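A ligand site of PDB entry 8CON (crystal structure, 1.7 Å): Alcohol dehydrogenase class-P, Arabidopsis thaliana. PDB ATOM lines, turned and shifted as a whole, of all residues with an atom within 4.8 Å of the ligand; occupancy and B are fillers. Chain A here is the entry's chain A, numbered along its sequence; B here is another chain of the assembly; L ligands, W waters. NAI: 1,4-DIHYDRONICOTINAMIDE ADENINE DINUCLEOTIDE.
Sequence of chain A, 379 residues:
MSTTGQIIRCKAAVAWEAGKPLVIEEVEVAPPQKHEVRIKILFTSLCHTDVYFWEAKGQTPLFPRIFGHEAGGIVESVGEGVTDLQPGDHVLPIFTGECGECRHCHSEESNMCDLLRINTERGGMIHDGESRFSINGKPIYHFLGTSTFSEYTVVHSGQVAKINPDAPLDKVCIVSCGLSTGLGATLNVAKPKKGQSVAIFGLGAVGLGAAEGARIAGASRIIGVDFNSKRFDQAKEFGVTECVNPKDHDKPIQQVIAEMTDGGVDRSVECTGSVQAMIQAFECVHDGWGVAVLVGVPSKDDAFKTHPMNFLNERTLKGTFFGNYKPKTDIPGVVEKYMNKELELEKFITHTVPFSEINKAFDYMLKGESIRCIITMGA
Water W4 lies within hydrogen-bond range of O2N of the ligand (2.6 Å), O of Cys 271 (3.0 Å), N of Gly 204 (3.0 Å) and N of Gly 207 (3.0 Å).
Water W8 bridges an oxygen (O2D) of the ligand (2.7 Å) and the side-chain hydroxyl of Thr 49 (2.8 Å).
Water W2 bridges O1N of the ligand (2.8 Å) and NH2 of Arg 372 (2.9 Å).
Water W6 lies within hydrogen-bond range of O1N of the ligand (2.8 Å), NH1 of Arg 372 (2.9 Å) and N of Ala 205 (3.2 Å).
Water W7 bridges NE of Arg 231 and O2A of the ligand.
Water W5 bridges ND1 of His 48 (2.5 Å) and O1N of the ligand (3.0 Å).
Residues that only touch the ligand: Cys 177 (3.98 Å), Thr 181 (3.5 Å), Gly 202 (3.3 Å), Leu 203 (3.97 Å), Gly 204 (3.4 Å), Phe 227 (3.4 Å), Asn 228 (3.97 Å), Arg 231 (3.4 Å), Cys 271 (3.1 Å), Thr 272 (3.6 Å), Gly 273 (3.6 Å), Ser 274 (3.6 Å), Gly 296 (3.5 Å) and Phe 321 (3.3 Å).
Hydrophobic or aromatic side chains within 4 Å of the ligand: His 48, Val 206, Phe 227, Val 295, Val 297 and Phe 321.
22 residues have an atom within 4 Å of the ligand: His 48, Cys 177, Thr 181, Gly 202, Leu 203, Gly 204, Ala 205, Val 206, Asp 226, Phe 227, Asn 228, Arg 231, Cys 271, Thr 272, Gly 273, Ser 274, Val 295, Gly 296, Val 297, Thr 320, Phe 321 and Phe 322.
An oxygen (O3B) of the ligand is in hydrogen-bond range of the side-chain carboxylate of Asp 226 (2.5 Å).
An oxygen (O7N) of the ligand is in hydrogen-bond range of the backbone NH (N) of Phe 322, at 2.7 Å.
O of Val 295 lies within hydrogen-bond range of N7N of the ligand (2.9 Å).
The backbone NH (N) of Val 206 is in hydrogen-bond range of an oxygen (O2N) of the ligand.
O3D of the ligand sits at hydrogen-bond distance from N of Val 297.
O1A of the ligand sits close to ND1 of His 48.
The backbone carbonyl oxygen (O) of Thr 320 is in hydrogen-bond range of a nitrogen (N7N) of the ligand (3.1 Å).
O2N of the ligand sits at hydrogen-bond distance from N of Ala 205 (3.2 Å).
N of Leu 203 sits at hydrogen-bond distance from OD2 of Asp 226 (3.0 Å).
The side-chain carboxylate (OD1) of Asp 226 is in hydrogen-bond range of the backbone NH (N) of Asn 228 (2.8 Å).
The backbone NH (N) of Gly 202 sits at hydrogen-bond distance from the backbone carbonyl oxygen (O) of Val 225, 2.7 Å away.
The backbone carbonyl oxygen of Leu 203 lies within hydrogen-bond range of the guanidinium group of Arg 231, at 3.4 Å.
The side-chain hydroxyl of Thr 181 is in hydrogen-bond range of the backbone carbonyl oxygen of Cys 177 (2.7 Å).
The side-chain hydroxyl (OG1) of Thr 272 sits at hydrogen-bond distance from the backbone NH (N) of Ser 274, at 2.8 Å.
OG of Ser 274 lies within hydrogen-bond range of N of Ala 277 (3.3 Å).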
ATOM      1  N   HIS A  48      -1.159  -2.343 -12.536  1.00  0.00           N
ATOM      2  CA  HIS A  48      -0.684  -3.646 -12.992  1.00  0.00           C
ATOM      3  C   HIS A  48       0.838  -3.748 -12.957  1.00  0.00           C
ATOM      4  O   HIS A  48       1.368  -4.857 -12.827  1.00  0.00           O
ATOM      5  CB  HIS A  48      -1.210  -3.910 -14.405  1.00  0.00           C
ATOM      6  CG  HIS A  48      -2.629  -4.368 -14.427  1.00  0.00           C
ATOM      7  ND1 HIS A  48      -3.628  -3.657 -15.065  1.00  0.00           N
ATOM      8  CD2 HIS A  48      -3.221  -5.471 -13.919  1.00  0.00           C
ATOM      9  CE1 HIS A  48      -4.776  -4.290 -14.920  1.00  0.00           C
ATOM     10  NE2 HIS A  48      -4.555  -5.404 -14.238  1.00  0.00           N
ATOM     11  N   THR A  49       1.546  -2.615 -13.068  1.00  0.00           N
ATOM     12  CA  THR A  49       3.004  -2.647 -12.994  1.00  0.00           C
ATOM     13  C   THR A  49       3.458  -3.137 -11.624  1.00  0.00           C
ATOM     14  O   THR A  49       4.364  -3.968 -11.534  1.00  0.00           O
ATOM     15  CB  THR A  49       3.569  -1.252 -13.289  1.00  0.00           C
ATOM     16  OG1 THR A  49       3.278  -0.915 -14.653  1.00  0.00           O
ATOM     17  CG2 THR A  49       5.071  -1.233 -13.072  1.00  0.00           C
ATOM     18  N   PHE A  95       8.159   7.185 -11.436  1.00  0.00           N
ATOM     19  CA  PHE A  95       8.974   6.006 -11.723  1.00  0.00           C
ATOM     20  C   PHE A  95      10.129   6.250 -12.720  1.00  0.00           C
ATOM     21  O   PHE A  95      10.861   5.321 -13.086  1.00  0.00           O
ATOM     22  CB  PHE A  95       8.060   4.841 -12.167  1.00  0.00           C
ATOM     23  CG  PHE A  95       7.383   5.023 -13.512  1.00  0.00           C
ATOM     24  CD1 PHE A  95       7.520   6.161 -14.284  1.00  0.00           C
ATOM     25  CD2 PHE A  95       6.512   4.045 -13.960  1.00  0.00           C
ATOM     26  CE1 PHE A  95       6.861   6.295 -15.504  1.00  0.00           C
ATOM     27  CE2 PHE A  95       5.850   4.166 -15.178  1.00  0.00           C
ATOM     28  CZ  PHE A  95       6.031   5.291 -15.937  1.00  0.00           C
ATOM     29  N   CYS A 177       1.476   7.910 -13.823  1.00  0.00           N
ATOM     30  CA  CYS A 177       1.585   6.661 -14.586  1.00  0.00           C
ATOM     31  C   CYS A 177       0.626   6.642 -15.772  1.00  0.00           C
ATOM     32  O   CYS A 177       0.842   7.329 -16.765  1.00  0.00           O
ATOM     33  CB  CYS A 177       1.330   5.469 -13.669  1.00  0.00           C
ATOM     34  SG  CYS A 177       1.548   3.834 -14.459  1.00  0.00           S
ATOM     35  N   GLY A 178      -0.475   5.886 -15.645  1.00  0.00           N
ATOM     36  CA  GLY A 178      -1.295   5.588 -16.821  1.00  0.00           C
ATOM     37  C   GLY A 178      -1.951   6.809 -17.447  1.00  0.00           C
ATOM     38  O   GLY A 178      -2.013   6.918 -18.679  1.00  0.00           O
ATOM     39  N   THR A 181       0.573   8.938 -19.315  1.00  0.00           N
ATOM     40  CA  THR A 181       1.133   8.182 -20.424  1.00  0.00           C
ATOM     41  C   THR A 181       0.191   8.189 -21.619  1.00  0.00           C
ATOM     42  O   THR A 181       0.598   8.452 -22.754  1.00  0.00           O
ATOM     43  CB  THR A 181       1.449   6.756 -19.986  1.00  0.00           C
ATOM     44  OG1 THR A 181       2.423   6.773 -18.939  1.00  0.00           O
ATOM     45  CG2 THR A 181       1.971   5.943 -21.153  1.00  0.00           C
ATOM     46  N   GLY A 202      -7.569  -0.875 -25.928  1.00  0.00           N
ATOM     47  CA  GLY A 202      -7.368  -0.984 -24.496  1.00  0.00           C
ATOM     48  C   GLY A 202      -7.971   0.200 -23.767  1.00  0.00           C
ATOM     49  O   GLY A 202      -7.622   1.350 -24.031  1.00  0.00           O
ATOM     50  N   LEU A 203      -8.888  -0.071 -22.825  1.00  0.00           N
ATOM     51  CA  LEU A 203      -9.604   0.976 -22.127  1.00  0.00           C
ATOM     52  C   LEU A 203      -9.377   0.899 -20.620  1.00  0.00           C
ATOM     53  O   LEU A 203     -10.279   1.165 -19.822  1.00  0.00           O
ATOM     54  CB  LEU A 203     -11.096   0.908 -22.457  1.00  0.00           C
ATOM     55  CG  LEU A 203     -11.351   1.156 -23.946  1.00  0.00           C
ATOM     56  CD1 LEU A 203     -12.783   0.808 -24.318  1.00  0.00           C
ATOM     57  CD2 LEU A 203     -10.990   2.575 -24.368  1.00  0.00           C
ATOM     58  N   GLY A 204      -8.174   0.494 -20.218  1.00  0.00           N
ATOM     59  CA  GLY A 204      -7.695   0.736 -18.881  1.00  0.00           C
ATOM     60  C   GLY A 204      -7.285   2.191 -18.731  1.00  0.00           C
ATOM     61  O   GLY A 204      -7.549   3.043 -19.583  1.00  0.00           O
ATOM     62  N   ALA A 205      -6.584   2.470 -17.631  1.00  0.00           N
ATOM     63  CA  ALA A 205      -6.214   3.846 -17.327  1.00  0.00           C
ATOM     64  C   ALA A 205      -5.424   4.490 -18.464  1.00  0.00           C
ATOM     65  O   ALA A 205      -5.593   5.679 -18.753  1.00  0.00           O
ATOM     66  CB  ALA A 205      -5.408   3.906 -16.026  1.00  0.00           C
ATOM     67  N   VAL A 206      -4.550   3.718 -19.122  1.00  0.00           N
ATOM     68  CA  VAL A 206      -3.780   4.304 -20.226  1.00  0.00           C
ATOM     69  C   VAL A 206      -4.706   4.686 -21.374  1.00  0.00           C
ATOM     70  O   VAL A 206      -4.679   5.820 -21.852  1.00  0.00           O
ATOM     71  CB  VAL A 206      -2.661   3.343 -20.684  1.00  0.00           C
ATOM     72  CG1 VAL A 206      -1.968   3.873 -21.949  1.00  0.00           C
ATOM     73  CG2 VAL A 206      -1.637   3.157 -19.577  1.00  0.00           C
ATOM     74  N   GLY A 207      -5.576   3.762 -21.791  1.00  0.00           N
ATOM     75  CA  GLY A 207      -6.479   4.074 -22.892  1.00  0.00           C
ATOM     76  C   GLY A 207      -7.446   5.201 -22.554  1.00  0.00           C
ATOM     77  O   GLY A 207      -7.776   6.026 -23.419  1.00  0.00           O
ATOM     78  N   VAL A 225     -11.605   0.284 -28.347  1.00  0.00           N
ATOM     79  CA  VAL A 225     -11.562  -1.146 -28.642  1.00  0.00           C
ATOM     80  C   VAL A 225     -11.099  -1.888 -27.401  1.00  0.00           C
ATOM     81  O   VAL A 225     -10.068  -1.539 -26.820  1.00  0.00           O
ATOM     82  CB  VAL A 225     -10.627  -1.456 -29.829  1.00  0.00           C
ATOM     83  CG1 VAL A 225     -10.541  -2.950 -30.054  1.00  0.00           C
ATOM     84  CG2 VAL A 225     -11.089  -0.722 -31.082  1.00  0.00           C
ATOM     85  N   ASP A 226     -11.832  -2.940 -27.016  1.00  0.00           N
ATOM     86  CA  ASP A 226     -11.422  -3.718 -25.859  1.00  0.00           C
ATOM     87  C   ASP A 226     -12.187  -5.041 -25.860  1.00  0.00           C
ATOM     88  O   ASP A 226     -13.361  -5.089 -26.228  1.00  0.00           O
ATOM     89  CB  ASP A 226     -11.668  -2.947 -24.555  1.00  0.00           C
ATOM     90  CG  ASP A 226     -10.878  -3.499 -23.372  1.00  0.00           C
ATOM     91  OD1 ASP A 226     -10.898  -4.731 -23.148  1.00  0.00           O
ATOM     92  OD2 ASP A 226     -10.220  -2.702 -22.676  1.00  0.00           O
ATOM     93  N   PHE A 227     -11.493  -6.117 -25.454  1.00  0.00           N
ATOM     94  CA  PHE A 227     -12.126  -7.418 -25.263  1.00  0.00           C
ATOM     95  C   PHE A 227     -13.181  -7.380 -24.167  1.00  0.00           C
ATOM     96  O   PHE A 227     -14.050  -8.267 -24.133  1.00  0.00           O
ATOM     97  CB  PHE A 227     -11.085  -8.471 -24.887  1.00  0.00           C
ATOM     98  CG  PHE A 227     -10.219  -8.923 -26.026  1.00  0.00           C
ATOM     99  CD1 PHE A 227     -10.594  -8.712 -27.347  1.00  0.00           C
ATOM    100  CD2 PHE A 227      -9.026  -9.587 -25.777  1.00  0.00           C
ATOM    101  CE1 PHE A 227      -9.784  -9.140 -28.395  1.00  0.00           C
ATOM    102  CE2 PHE A 227      -8.218 -10.021 -26.812  1.00  0.00           C
ATOM    103  CZ  PHE A 227      -8.595  -9.801 -28.122  1.00  0.00           C
ATOM    104  N   ASN A 228     -13.117  -6.395 -23.278  1.00  0.00           N
ATOM    105  CA  ASN A 228     -13.958  -6.343 -22.084  1.00  0.00           C
ATOM    106  C   ASN A 228     -15.038  -5.289 -22.287  1.00  0.00           C
ATOM    107  O   ASN A 228     -14.774  -4.083 -22.193  1.00  0.00           O
ATOM    108  CB  ASN A 228     -13.103  -6.024 -20.858  1.00  0.00           C
ATOM    109  CG  ASN A 228     -13.898  -6.078 -19.571  1.00  0.00           C
ATOM    110  OD1 ASN A 228     -15.121  -6.069 -19.588  1.00  0.00           O
ATOM    111  ND2 ASN A 228     -13.199  -6.126 -18.439  1.00  0.00           N
ATOM    112  N   ARG A 231     -15.976  -2.281 -19.848  1.00  0.00           N
ATOM    113  CA  ARG A 231     -15.193  -1.021 -19.799  1.00  0.00           C
ATOM    114  C   ARG A 231     -15.774   0.051 -20.731  1.00  0.00           C
ATOM    115  O   ARG A 231     -15.250   1.161 -20.700  1.00  0.00           O
ATOM    116  CB  ARG A 231     -13.739  -1.326 -20.167  1.00  0.00           C
ATOM    117  CG  ARG A 231     -13.045  -2.291 -19.224  1.00  0.00           C
ATOM    118  CD  ARG A 231     -11.636  -1.821 -18.956  1.00  0.00           C
ATOM    119  NE  ARG A 231     -11.084  -2.347 -17.718  1.00  0.00           N
ATOM    120  CZ  ARG A 231     -10.671  -1.596 -16.709  1.00  0.00           C
ATOM    121  NH1 ARG A 231     -10.733  -0.273 -16.787  1.00  0.00           N
ATOM    122  NH2 ARG A 231     -10.173  -2.165 -15.621  1.00  0.00           N
ATOM    123  N   PRO A 246     -13.756  -6.740 -30.241  1.00  0.00           N
ATOM    124  CA  PRO A 246     -13.326  -7.647 -31.328  1.00  0.00           C
ATOM    125  C   PRO A 246     -14.053  -8.974 -31.313  1.00  0.00           C
ATOM    126  O   PRO A 246     -14.295  -9.548 -32.386  1.00  0.00           O
ATOM    127  CB  PRO A 246     -11.821  -7.818 -31.074  1.00  0.00           C
ATOM    128  CG  PRO A 246     -11.433  -6.602 -30.266  1.00  0.00           C
ATOM    129  CD  PRO A 246     -12.617  -6.317 -29.404  1.00  0.00           C
ATOM    130  N   CYS A 271      -2.859   0.506 -26.396  1.00  0.00           N
ATOM    131  CA  CYS A 271      -2.764   0.652 -24.944  1.00  0.00           C
ATOM    132  C   CYS A 271      -3.079  -0.667 -24.238  1.00  0.00           C
ATOM    133  O   CYS A 271      -3.657  -0.672 -23.153  1.00  0.00           O
ATOM    134  CB  CYS A 271      -3.727   1.730 -24.452  1.00  0.00           C
ATOM    135  SG  CYS A 271      -3.509   3.367 -25.211  1.00  0.00           S
ATOM    136  N   THR A 272      -2.705  -1.798 -24.852  1.00  0.00           N
ATOM    137  CA  THR A 272      -3.004  -3.122 -24.319  1.00  0.00           C
ATOM    138  C   THR A 272      -1.787  -3.864 -23.813  1.00  0.00           C
ATOM    139  O   THR A 272      -1.885  -4.606 -22.830  1.00  0.00           O
ATOM    140  CB  THR A 272      -3.681  -3.990 -25.389  1.00  0.00           C
ATOM    141  OG1 THR A 272      -2.721  -4.335 -26.388  1.00  0.00           O
ATOM    142  CG2 THR A 272      -4.824  -3.259 -26.039  1.00  0.00           C
ATOM    143  N   GLY A 273      -0.639  -3.715 -24.473  1.00  0.00           N
ATOM    144  CA  GLY A 273       0.489  -4.578 -24.232  1.00  0.00           C
ATOM    145  C   GLY A 273       0.501  -5.829 -25.081  1.00  0.00           C
ATOM    146  O   GLY A 273       1.478  -6.581 -25.027  1.00  0.00           O
ATOM    147  N   SER A 274      -0.545  -6.088 -25.856  1.00  0.00           N
ATOM    148  CA  SER A 274      -0.602  -7.258 -26.720  1.00  0.00           C
ATOM    149  C   SER A 274       0.087  -6.934 -28.043  1.00  0.00           C
ATOM    150  O   SER A 274      -0.285  -5.969 -28.716  1.00  0.00           O
ATOM    151  CB  SER A 274      -2.055  -7.676 -26.969  1.00  0.00           C
ATOM    152  OG  SER A 274      -2.156  -8.509 -28.110  1.00  0.00           O
ATOM    153  N   ALA A 277      -2.220  -6.688 -30.817  1.00  0.00           N
ATOM    154  CA  ALA A 277      -2.901  -5.414 -30.882  1.00  0.00           C
ATOM    155  C   ALA A 277      -2.007  -4.319 -31.453  1.00  0.00           C
ATOM    156  O   ALA A 277      -2.510  -3.362 -32.043  1.00  0.00           O
ATOM    157  CB  ALA A 277      -3.401  -4.985 -29.504  1.00  0.00           C
ATOM    158  N   VAL A 295       2.011   1.994 -27.062  1.00  0.00           N
ATOM    159  CA  VAL A 295       2.162   2.399 -25.666  1.00  0.00           C
ATOM    160  C   VAL A 295       2.302   1.184 -24.756  1.00  0.00           C
ATOM    161  O   VAL A 295       3.134   1.167 -23.829  1.00  0.00           O
ATOM    162  CB  VAL A 295       0.999   3.295 -25.208  1.00  0.00           C
ATOM    163  CG1 VAL A 295       1.308   3.910 -23.848  1.00  0.00           C
ATOM    164  CG2 VAL A 295       0.690   4.382 -26.223  1.00  0.00           C
ATOM    165  N   GLY A 296       1.477   0.164 -24.981  1.00  0.00           N
ATOM    166  CA  GLY A 296       1.506  -1.003 -24.109  1.00  0.00           C
ATOM    167  C   GLY A 296       2.864  -1.688 -24.112  1.00  0.00           C
ATOM    168  O   GLY A 296       3.619  -1.612 -25.083  1.00  0.00           O
ATOM    169  N   VAL A 297       3.181  -2.343 -23.004  1.00  0.00           N
ATOM    170  CA  VAL A 297       4.445  -3.048 -22.841  1.00  0.00           C
ATOM    171  C   VAL A 297       4.208  -4.538 -23.083  1.00  0.00           C
ATOM    172  O   VAL A 297       3.332  -5.118 -22.437  1.00  0.00           O
ATOM    173  CB  VAL A 297       5.070  -2.814 -21.440  1.00  0.00           C
ATOM    174  CG1 VAL A 297       6.350  -3.629 -21.282  1.00  0.00           C
ATOM    175  CG2 VAL A 297       5.371  -1.344 -21.240  1.00  0.00           C
ATOM    176  N   THR A 320       5.899   5.445 -27.398  1.00  0.00           N
ATOM    177  CA  THR A 320       6.028   6.424 -26.330  1.00  0.00           C
ATOM    178  C   THR A 320       6.438   5.775 -25.022  1.00  0.00           C
ATOM    179  O   THR A 320       6.054   4.642 -24.720  1.00  0.00           O
ATOM    180  CB  THR A 320       4.742   7.234 -26.121  1.00  0.00           C
ATOM    181  OG1 THR A 320       5.017   8.323 -25.245  1.00  0.00           O
ATOM    182  CG2 THR A 320       3.633   6.374 -25.535  1.00  0.00           C
ATOM    183  N   PHE A 321       7.233   6.509 -24.256  1.00  0.00           N
ATOM    184  CA  PHE A 321       7.513   6.227 -22.855  1.00  0.00           C
ATOM    185  C   PHE A 321       6.898   7.357 -22.041  1.00  0.00           C
ATOM    186  O   PHE A 321       7.263   8.519 -22.225  1.00  0.00           O
ATOM    187  CB  PHE A 321       9.005   6.148 -22.564  1.00  0.00           C
ATOM    188  CG  PHE A 321       9.315   6.062 -21.095  1.00  0.00           C
ATOM    189  CD1 PHE A 321       8.669   5.103 -20.302  1.00  0.00           C
ATOM    190  CD2 PHE A 321      10.232   6.911 -20.510  1.00  0.00           C
ATOM    191  CE1 PHE A 321       8.936   5.020 -18.945  1.00  0.00           C
ATOM    192  CE2 PHE A 321      10.513   6.811 -19.149  1.00  0.00           C
ATOM    193  CZ  PHE A 321       9.848   5.868 -18.369  1.00  0.00           C
ATOM    194  N   PHE A 322       5.937   7.011 -21.198  1.00  0.00           N
ATOM    195  CA  PHE A 322       5.325   7.965 -20.270  1.00  0.00           C
ATOM    196  C   PHE A 322       4.787   9.184 -21.017  1.00  0.00           C
ATOM    197  O   PHE A 322       4.888  10.322 -20.559  1.00  0.00           O
ATOM    198  CB  PHE A 322       6.330   8.341 -19.171  1.00  0.00           C
ATOM    199  CG  PHE A 322       5.758   9.125 -18.014  1.00  0.00           C
ATOM    200  CD1 PHE A 322       4.616   8.673 -17.347  1.00  0.00           C
ATOM    201  CD2 PHE A 322       6.414  10.252 -17.548  1.00  0.00           C
ATOM    202  CE1 PHE A 322       4.118   9.395 -16.278  1.00  0.00           C
ATOM    203  CE2 PHE A 322       5.926  10.965 -16.471  1.00  0.00           C
ATOM    204  CZ  PHE A 322       4.763  10.535 -15.841  1.00  0.00           C
ATOM    205  N   ARG A 372      -8.513   2.797 -10.677  1.00  0.00           N
ATOM    206  CA  ARG A 372      -7.579   3.060  -9.597  1.00  0.00           C
ATOM    207  C   ARG A 372      -8.249   2.981  -8.235  1.00  0.00           C
ATOM    208  O   ARG A 372      -9.422   3.348  -8.054  1.00  0.00           O
ATOM    209  CB  ARG A 372      -6.899   4.416  -9.745  1.00  0.00           C
ATOM    210  CG  ARG A 372      -5.824   4.412 -10.829  1.00  0.00           C
ATOM    211  CD  ARG A 372      -4.644   3.506 -10.434  1.00  0.00           C
ATOM    212  NE  ARG A 372      -3.519   3.684 -11.349  1.00  0.00           N
ATOM    213  CZ  ARG A 372      -3.477   3.215 -12.589  1.00  0.00           C
ATOM    214  NH1 ARG A 372      -4.503   2.561 -13.118  1.00  0.00           N
ATOM    215  NH2 ARG A 372      -2.370   3.393 -13.319  1.00  0.00           N
ATOM    216  N   LEU B 312       8.846   1.827 -27.972  1.00  0.00           N
ATOM    217  CA  LEU B 312       8.627   2.389 -26.641  1.00  0.00           C
ATOM    218  C   LEU B 312       9.814   3.208 -26.159  1.00  0.00           C
ATOM    219  O   LEU B 312       9.645   4.088 -25.303  1.00  0.00           O
ATOM    220  CB  LEU B 312       8.325   1.269 -25.650  1.00  0.00           C
ATOM    221  CG  LEU B 312       7.025   0.503 -25.916  1.00  0.00           C
ATOM    222  CD1 LEU B 312       6.546  -0.249 -24.677  1.00  0.00           C
ATOM    223  CD2 LEU B 312       5.947   1.433 -26.425  1.00  0.00           C
HETATM  224  PA  NAI L   1      -5.016  -2.499 -18.119  1.00  0.00           P
HETATM  225  O1A NAI L   1      -4.715  -3.930 -17.971  1.00  0.00           O
HETATM  226  O2A NAI L   1      -5.796  -1.844 -16.982  1.00  0.00           O
HETATM  227  O5B NAI L   1      -5.806  -2.212 -19.448  1.00  0.00           O
HETATM  228  C5B NAI L   1      -5.597  -3.030 -20.623  1.00  0.00           C
HETATM  229  C4B NAI L   1      -6.923  -3.174 -21.315  1.00  0.00           C
HETATM  230  O4B NAI L   1      -6.729  -3.703 -22.647  1.00  0.00           O
HETATM  231  C3B NAI L   1      -7.915  -4.112 -20.615  1.00  0.00           C
HETATM  232  O3B NAI L   1      -9.180  -3.464 -20.566  1.00  0.00           O
HETATM  233  C2B NAI L   1      -7.910  -5.372 -21.494  1.00  0.00           C
HETATM  234  O2B NAI L   1      -9.182  -5.986 -21.491  1.00  0.00           O
HETATM  235  C1B NAI L   1      -7.625  -4.770 -22.870  1.00  0.00           C
HETATM  236  N9A NAI L   1      -7.000  -5.671 -23.828  1.00  0.00           N
HETATM  237  C8A NAI L   1      -5.973  -6.557 -23.605  1.00  0.00           C
HETATM  238  N7A NAI L   1      -5.582  -7.198 -24.683  1.00  0.00           N
HETATM  239  C5A NAI L   1      -6.389  -6.682 -25.680  1.00  0.00           C
HETATM  240  C6A NAI L   1      -6.469  -6.946 -27.069  1.00  0.00           C
HETATM  241  N6A NAI L   1      -5.710  -7.835 -27.703  1.00  0.00           N
HETATM  242  N1A NAI L   1      -7.380  -6.256 -27.781  1.00  0.00           N
HETATM  243  C2A NAI L   1      -8.156  -5.365 -27.150  1.00  0.00           C
HETATM  244  N3A NAI L   1      -8.173  -5.039 -25.861  1.00  0.00           N
HETATM  245  C4A NAI L   1      -7.265  -5.737 -25.170  1.00  0.00           C
HETATM  246  O3  NAI L   1      -3.665  -1.672 -18.319  1.00  0.00           O
HETATM  247  PN  NAI L   1      -3.223  -0.140 -18.285  1.00  0.00           P
HETATM  248  O1N NAI L   1      -2.822   0.196 -16.849  1.00  0.00           O
HETATM  249  O2N NAI L   1      -4.190   0.716 -18.932  1.00  0.00           O
HETATM  250  O5D NAI L   1      -1.887  -0.246 -19.135  1.00  0.00           O
HETATM  251  C5D NAI L   1      -1.948  -0.424 -20.568  1.00  0.00           C
HETATM  252  C4D NAI L   1      -0.581  -0.823 -21.070  1.00  0.00           C
HETATM  253  O4D NAI L   1       0.301   0.326 -21.052  1.00  0.00           O
HETATM  254  C3D NAI L   1       0.125  -1.912 -20.272  1.00  0.00           C
HETATM  255  O3D NAI L   1       0.827  -2.801 -21.134  1.00  0.00           O
HETATM  256  C2D NAI L   1       1.114  -1.113 -19.422  1.00  0.00           C
HETATM  257  O2D NAI L   1       2.210  -1.910 -19.002  1.00  0.00           O
HETATM  258  C1D NAI L   1       1.521  -0.063 -20.449  1.00  0.00           C
HETATM  259  N1N NAI L   1       2.166   1.118 -19.892  1.00  0.00           N
HETATM  260  C2N NAI L   1       3.152   1.734 -20.589  1.00  0.00           C
HETATM  261  C3N NAI L   1       3.674   2.917 -20.196  1.00  0.00           C
HETATM  262  C7N NAI L   1       4.656   3.543 -21.080  1.00  0.00           C
HETATM  263  O7N NAI L   1       5.441   4.401 -20.666  1.00  0.00           O
HETATM  264  N7N NAI L   1       4.646   3.172 -22.355  1.00  0.00           N
HETATM  265  C4N NAI L   1       3.431   3.451 -18.820  1.00  0.00           C
HETATM  266  C5N NAI L   1       2.229   2.777 -18.240  1.00  0.00           C
HETATM  267  C6N NAI L   1       1.770   1.601 -18.686  1.00  0.00           C
HETATM  268  O   HOH W   1      -1.674  -4.688 -18.115  1.00  0.00           O
HETATM  269  O   HOH W   2      -1.531   2.450 -15.875  1.00  0.00           O
HETATM  270  O   HOH W   3       0.115   0.212 -15.810  1.00  0.00           O
HETATM  271  O   HOH W   4      -5.394   0.771 -21.254  1.00  0.00           O
HETATM  272  O   HOH W   5      -3.325  -1.265 -14.254  1.00  0.00           O
HETATM  273  O   HOH W   6      -5.105   0.781 -15.288  1.00  0.00           O
HETATM  274  O   HOH W   7      -8.401  -2.841 -17.704  1.00  0.00           O
HETATM  275  O   HOH W   8       1.646  -2.431 -16.374  1.00  0.00           O
HETATM  276  O   HOH W   9      -7.758  -6.373 -30.657  1.00  0.00           O
